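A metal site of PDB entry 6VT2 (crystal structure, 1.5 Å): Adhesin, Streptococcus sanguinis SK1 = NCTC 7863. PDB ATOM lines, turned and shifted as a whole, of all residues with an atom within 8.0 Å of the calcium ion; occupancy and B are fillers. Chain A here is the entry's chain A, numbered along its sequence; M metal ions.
N of Ser 307 lies within hydrogen-bond range of OD1 of Asp 305, at 3.0 Å. The side-chain carboxylate of Asp 305 is in hydrogen-bond range of the backbone NH of Gly 308 (3.2 Å). The backbone NH of Asp 201 sits at hydrogen-bond distance from the backbone carbonyl oxygen of Val 141, 2.8 Å away. The side-chain carboxylate (OD1) of Asp 305 is in hydrogen-bond range of the backbone NH (N) of Leu 309. OD2 of Asp 230 lies close to OG of Ser 232 (2.6 Å).
Five residues have an atom within 4 Å of the calcium ion: Asp 201, Val 203, Asp 230, Asn 231 and Asp 305. The nearest printed residue that does not touch the calcium ion is Ser 232 (4.3 Å).
The calcium ion is bound by the backbone carbonyl oxygen (O) of Val 203 (2.3 Å), the side-chain carboxylate (OD2) of Asp 305 (2.4 Å), the side-chain amide oxygen (OD1) of Asn 231 (2.4 Å), the side-chain carboxylate (OD1) of Asp 201 (2.4 Å), the side-chain carboxylate (OD2) of Asp 230 (2.5 Å), the side-chain carboxylate (OD1) of Asp 230 (2.5 Å) and the side-chain carboxylate (OD2) of Asp 201 (2.5 Å). The calcium ion has seven donor atoms within binding distance.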
ATOM      1  N   TYR A 140     -18.814   6.222  -7.132  1.00  0.00           N
ATOM      2  CA  TYR A 140     -18.675   5.733  -8.498  1.00  0.00           C
ATOM      3  C   TYR A 140     -17.212   5.539  -8.817  1.00  0.00           C
ATOM      4  O   TYR A 140     -16.407   6.444  -8.628  1.00  0.00           O
ATOM      5  CB  TYR A 140     -19.314   6.715  -9.475  1.00  0.00           C
ATOM      6  CG  TYR A 140     -20.802   6.644  -9.466  1.00  0.00           C
ATOM      7  CD1 TYR A 140     -21.459   5.683 -10.215  1.00  0.00           C
ATOM      8  CD2 TYR A 140     -21.575   7.457  -8.645  1.00  0.00           C
ATOM      9  CE1 TYR A 140     -22.815   5.571 -10.209  1.00  0.00           C
ATOM     10  CE2 TYR A 140     -22.939   7.335  -8.636  1.00  0.00           C
ATOM     11  CZ  TYR A 140     -23.558   6.387  -9.429  1.00  0.00           C
ATOM     12  OH  TYR A 140     -24.922   6.257  -9.413  1.00  0.00           O
ATOM     13  N   VAL A 141     -16.856   4.336  -9.292  1.00  0.00           N
ATOM     14  CA  VAL A 141     -15.470   3.984  -9.483  1.00  0.00           C
ATOM     15  C   VAL A 141     -15.258   3.440 -10.894  1.00  0.00           C
ATOM     16  O   VAL A 141     -16.191   3.020 -11.584  1.00  0.00           O
ATOM     17  CB  VAL A 141     -15.013   2.949  -8.426  1.00  0.00           C
ATOM     18  CG1 VAL A 141     -15.245   3.508  -7.014  1.00  0.00           C
ATOM     19  CG2 VAL A 141     -15.717   1.657  -8.569  1.00  0.00           C
ATOM     20  N   THR A 200     -19.987   1.053 -10.922  1.00  0.00           N
ATOM     21  CA  THR A 200     -19.148   1.465 -12.028  1.00  0.00           C
ATOM     22  C   THR A 200     -19.581   2.817 -12.524  1.00  0.00           C
ATOM     23  O   THR A 200     -20.782   3.026 -12.726  1.00  0.00           O
ATOM     24  CB  THR A 200     -19.247   0.487 -13.170  1.00  0.00           C
ATOM     25  OG1 THR A 200     -19.194  -0.843 -12.638  1.00  0.00           O
ATOM     26  CG2 THR A 200     -18.079   0.681 -14.124  1.00  0.00           C
ATOM     27  N   ASP A 201     -18.632   3.717 -12.714  1.00  0.00           N
ATOM     28  CA  ASP A 201     -18.922   4.979 -13.391  1.00  0.00           C
ATOM     29  C   ASP A 201     -18.922   4.682 -14.872  1.00  0.00           C
ATOM     30  O   ASP A 201     -17.870   4.348 -15.431  1.00  0.00           O
ATOM     31  CB  ASP A 201     -17.919   6.072 -13.076  1.00  0.00           C
ATOM     32  CG  ASP A 201     -18.403   7.465 -13.457  1.00  0.00           C
ATOM     33  OD1 ASP A 201     -19.260   7.587 -14.342  1.00  0.00           O
ATOM     34  OD2 ASP A 201     -17.918   8.402 -12.782  1.00  0.00           O
ATOM     35  N   ARG A 202     -20.068   4.834 -15.488  1.00  0.00           N
ATOM     36  CA  ARG A 202     -20.273   4.619 -16.907  1.00  0.00           C
ATOM     37  C   ARG A 202     -20.784   5.837 -17.635  1.00  0.00           C
ATOM     38  O   ARG A 202     -21.199   5.734 -18.806  1.00  0.00           O
ATOM     39  CB  ARG A 202     -21.263   3.470 -17.138  1.00  0.00           C
ATOM     40  CG  ARG A 202     -20.861   2.195 -16.478  1.00  0.00           C
ATOM     41  CD  ARG A 202     -21.961   1.118 -16.732  1.00  0.00           C
ATOM     42  NE  ARG A 202     -23.212   1.447 -16.056  1.00  0.00           N
ATOM     43  CZ  ARG A 202     -24.367   1.706 -16.665  1.00  0.00           C
ATOM     44  NH1 ARG A 202     -24.461   1.714 -17.990  1.00  0.00           N
ATOM     45  NH2 ARG A 202     -25.436   1.984 -15.934  1.00  0.00           N
ATOM     46  N   VAL A 203     -20.785   6.984 -17.002  1.00  0.00           N
ATOM     47  CA  VAL A 203     -21.354   8.204 -17.584  1.00  0.00           C
ATOM     48  C   VAL A 203     -20.286   9.280 -17.544  1.00  0.00           C
ATOM     49  O   VAL A 203     -19.775   9.592 -16.464  1.00  0.00           O
ATOM     50  CB  VAL A 203     -22.602   8.636 -16.819  1.00  0.00           C
ATOM     51  CG1 VAL A 203     -23.248   9.804 -17.593  1.00  0.00           C
ATOM     52  CG2 VAL A 203     -23.573   7.476 -16.720  1.00  0.00           C
ATOM     53  N   ALA A 204     -19.965   9.831 -18.705  1.00  0.00           N
ATOM     54  CA  ALA A 204     -19.042  10.941 -18.753  1.00  0.00           C
ATOM     55  C   ALA A 204     -19.675  12.225 -18.215  1.00  0.00           C
ATOM     56  O   ALA A 204     -20.896  12.350 -18.103  1.00  0.00           O
ATOM     57  CB  ALA A 204     -18.584  11.205 -20.181  1.00  0.00           C
ATOM     58  N   PRO A 205     -18.849  13.202 -17.840  1.00  0.00           N
ATOM     59  CA  PRO A 205     -19.402  14.484 -17.392  1.00  0.00           C
ATOM     60  C   PRO A 205     -20.265  15.135 -18.467  1.00  0.00           C
ATOM     61  O   PRO A 205     -20.110  14.880 -19.655  1.00  0.00           O
ATOM     62  CB  PRO A 205     -18.157  15.324 -17.141  1.00  0.00           C
ATOM     63  CG  PRO A 205     -17.047  14.341 -16.823  1.00  0.00           C
ATOM     64  CD  PRO A 205     -17.393  13.148 -17.676  1.00  0.00           C
ATOM     65  N   VAL A 206     -21.131  16.024 -17.993  1.00  0.00           N
ATOM     66  CA  VAL A 206     -22.100  16.720 -18.792  1.00  0.00           C
ATOM     67  C   VAL A 206     -21.731  18.204 -18.784  1.00  0.00           C
ATOM     68  O   VAL A 206     -21.487  18.790 -17.716  1.00  0.00           O
ATOM     69  CB  VAL A 206     -23.520  16.546 -18.250  1.00  0.00           C
ATOM     70  CG1 VAL A 206     -24.472  17.445 -19.043  1.00  0.00           C
ATOM     71  CG2 VAL A 206     -23.929  15.115 -18.331  1.00  0.00           C
ATOM     72  N   TYR A 229     -21.274  19.052 -14.772  1.00  0.00           N
ATOM     73  CA  TYR A 229     -21.469  18.174 -13.632  1.00  0.00           C
ATOM     74  C   TYR A 229     -21.189  16.751 -14.071  1.00  0.00           C
ATOM     75  O   TYR A 229     -21.015  16.436 -15.234  1.00  0.00           O
ATOM     76  CB  TYR A 229     -22.875  18.283 -13.060  1.00  0.00           C
ATOM     77  CG  TYR A 229     -23.955  17.734 -13.919  1.00  0.00           C
ATOM     78  CD1 TYR A 229     -24.338  16.402 -13.801  1.00  0.00           C
ATOM     79  CD2 TYR A 229     -24.645  18.550 -14.819  1.00  0.00           C
ATOM     80  CE1 TYR A 229     -25.383  15.923 -14.575  1.00  0.00           C
ATOM     81  CE2 TYR A 229     -25.659  18.071 -15.581  1.00  0.00           C
ATOM     82  CZ  TYR A 229     -26.032  16.767 -15.463  1.00  0.00           C
ATOM     83  OH  TYR A 229     -27.045  16.308 -16.276  1.00  0.00           O
ATOM     84  N   ASP A 230     -21.032  15.906 -13.096  1.00  0.00           N
ATOM     85  CA  ASP A 230     -20.840  14.477 -13.395  1.00  0.00           C
ATOM     86  C   ASP A 230     -21.750  13.706 -12.450  1.00  0.00           C
ATOM     87  O   ASP A 230     -21.939  14.164 -11.355  1.00  0.00           O
ATOM     88  CB  ASP A 230     -19.371  14.084 -13.232  1.00  0.00           C
ATOM     89  CG  ASP A 230     -19.073  12.696 -13.721  1.00  0.00           C
ATOM     90  OD1 ASP A 230     -19.300  12.450 -14.829  1.00  0.00           O
ATOM     91  OD2 ASP A 230     -18.696  11.919 -12.870  1.00  0.00           O
ATOM     92  N   ASN A 231     -22.125  12.486 -12.802  1.00  0.00           N
ATOM     93  CA  ASN A 231     -22.935  11.607 -11.927  1.00  0.00           C
ATOM     94  C   ASN A 231     -22.165  11.252 -10.634  1.00  0.00           C
ATOM     95  O   ASN A 231     -22.772  11.070  -9.645  1.00  0.00           O
ATOM     96  CB  ASN A 231     -23.380  10.338 -12.668  1.00  0.00           C
ATOM     97  CG  ASN A 231     -22.233   9.446 -13.040  1.00  0.00           C
ATOM     98  OD1 ASN A 231     -21.185   9.920 -13.267  1.00  0.00           O
ATOM     99  ND2 ASN A 231     -22.415   8.150 -13.050  1.00  0.00           N
ATOM    100  N   SER A 232     -20.828  11.253 -10.637  1.00  0.00           N
ATOM    101  CA  SER A 232     -20.014  11.013  -9.430  1.00  0.00           C
ATOM    102  C   SER A 232     -19.967  12.258  -8.542  1.00  0.00           C
ATOM    103  O   SER A 232     -19.477  12.163  -7.446  1.00  0.00           O
ATOM    104  CB  SER A 232     -18.630  10.649  -9.761  1.00  0.00           C
ATOM    105  OG  SER A 232     -17.985  11.748 -10.365  1.00  0.00           O
ATOM    106  N   GLY A 233     -20.320  13.424  -9.086  1.00  0.00           N
ATOM    107  CA  GLY A 233     -20.193  14.660  -8.382  1.00  0.00           C
ATOM    108  C   GLY A 233     -18.815  15.260  -8.464  1.00  0.00           C
ATOM    109  O   GLY A 233     -18.588  16.295  -7.810  1.00  0.00           O
ATOM    110  N   LYS A 234     -17.912  14.673  -9.260  1.00  0.00           N
ATOM    111  CA  LYS A 234     -16.533  15.126  -9.319  1.00  0.00           C
ATOM    112  C   LYS A 234     -16.049  15.182 -10.760  1.00  0.00           C
ATOM    113  O   LYS A 234     -16.170  14.195 -11.511  1.00  0.00           O
ATOM    114  CB  LYS A 234     -15.636  14.205  -8.490  1.00  0.00           C
ATOM    115  CG  LYS A 234     -14.186  14.408  -8.663  1.00  0.00           C
ATOM    116  CD  LYS A 234     -13.730  15.826  -8.256  1.00  0.00           C
ATOM    117  CE  LYS A 234     -12.227  15.922  -8.325  1.00  0.00           C
ATOM    118  NZ  LYS A 234     -11.762  17.328  -8.285  1.00  0.00           N
ATOM    119  N   ILE A 235     -15.518  16.325 -11.145  1.00  0.00           N
ATOM    120  CA  ILE A 235     -14.779  16.484 -12.389  1.00  0.00           C
ATOM    121  C   ILE A 235     -13.344  16.834 -12.044  1.00  0.00           C
ATOM    122  O   ILE A 235     -13.079  17.656 -11.165  1.00  0.00           O
ATOM    123  CB  ILE A 235     -15.450  17.560 -13.269  1.00  0.00           C
ATOM    124  CG1 ILE A 235     -16.791  16.994 -13.738  1.00  0.00           C
ATOM    125  CG2 ILE A 235     -14.552  18.025 -14.352  1.00  0.00           C
ATOM    126  CD1 ILE A 235     -17.619  18.058 -14.453  1.00  0.00           C
ATOM    127  N   THR A 304     -13.526  15.559 -17.906  1.00  0.00           N
ATOM    128  CA  THR A 304     -13.183  14.221 -17.492  1.00  0.00           C
ATOM    129  C   THR A 304     -13.471  14.049 -16.006  1.00  0.00           C
ATOM    130  O   THR A 304     -13.237  14.966 -15.215  1.00  0.00           O
ATOM    131  CB  THR A 304     -11.701  13.986 -17.753  1.00  0.00           C
ATOM    132  OG1 THR A 304     -11.417  14.118 -19.137  1.00  0.00           O
ATOM    133  CG2 THR A 304     -11.294  12.536 -17.356  1.00  0.00           C
ATOM    134  N   ASP A 305     -14.027  12.893 -15.633  1.00  0.00           N
ATOM    135  CA  ASP A 305     -14.296  12.614 -14.228  1.00  0.00           C
ATOM    136  C   ASP A 305     -13.108  11.846 -13.637  1.00  0.00           C
ATOM    137  O   ASP A 305     -12.132  11.560 -14.316  1.00  0.00           O
ATOM    138  CB  ASP A 305     -15.654  11.905 -14.072  1.00  0.00           C
ATOM    139  CG  ASP A 305     -15.706  10.508 -14.685  1.00  0.00           C
ATOM    140  OD1 ASP A 305     -14.637   9.868 -14.801  1.00  0.00           O
ATOM    141  OD2 ASP A 305     -16.805  10.138 -15.077  1.00  0.00           O
ATOM    142  N   ALA A 306     -13.202  11.537 -12.339  1.00  0.00           N
ATOM    143  CA  ALA A 306     -12.044  10.966 -11.663  1.00  0.00           C
ATOM    144  C   ALA A 306     -11.805   9.525 -12.075  1.00  0.00           C
ATOM    145  O   ALA A 306     -10.695   9.002 -11.860  1.00  0.00           O
ATOM    146  CB  ALA A 306     -12.217  11.036 -10.164  1.00  0.00           C
ATOM    147  N   SER A 307     -12.808   8.870 -12.674  1.00  0.00           N
ATOM    148  CA  SER A 307     -12.634   7.516 -13.195  1.00  0.00           C
ATOM    149  C   SER A 307     -11.967   7.491 -14.552  1.00  0.00           C
ATOM    150  O   SER A 307     -11.720   6.411 -15.083  1.00  0.00           O
ATOM    151  CB  SER A 307     -13.979   6.799 -13.289  1.00  0.00           C
ATOM    152  OG  SER A 307     -14.538   6.631 -12.032  1.00  0.00           O
ATOM    153  N   GLY A 308     -11.693   8.655 -15.135  1.00  0.00           N
ATOM    154  CA  GLY A 308     -11.102   8.739 -16.450  1.00  0.00           C
ATOM    155  C   GLY A 308     -12.045   8.797 -17.624  1.00  0.00           C
ATOM    156  O   GLY A 308     -11.585   8.648 -18.773  1.00  0.00           O
ATOM    157  N   LEU A 309     -13.363   8.926 -17.391  1.00  0.00           N
ATOM    158  CA  LEU A 309     -14.297   9.048 -18.500  1.00  0.00           C
ATOM    159  C   LEU A 309     -14.283  10.500 -18.967  1.00  0.00           C
ATOM    160  O   LEU A 309     -14.488  11.411 -18.168  1.00  0.00           O
ATOM    161  CB  LEU A 309     -15.727   8.684 -18.121  1.00  0.00           C
ATOM    162  CG  LEU A 309     -16.016   7.229 -17.761  1.00  0.00           C
ATOM    163  CD1 LEU A 309     -17.485   7.112 -17.487  1.00  0.00           C
ATOM    164  CD2 LEU A 309     -15.543   6.288 -18.814  1.00  0.00           C
ATOM    165  N   THR A 310     -14.050  10.695 -20.258  1.00  0.00           N
ATOM    166  CA  THR A 310     -14.047  12.028 -20.859  1.00  0.00           C
ATOM    167  C   THR A 310     -15.255  12.157 -21.781  1.00  0.00           C
ATOM    168  O   THR A 310     -15.540  11.254 -22.584  1.00  0.00           O
ATOM    169  CB  THR A 310     -12.769  12.259 -21.624  1.00  0.00           C
ATOM    170  OG1 THR A 310     -11.649  12.101 -20.741  1.00  0.00           O
ATOM    171  CG2 THR A 310     -12.743  13.666 -22.222  1.00  0.00           C
HETATM  172 CA    CA M   1     -19.060   9.990 -14.365  1.00  0.00          CA
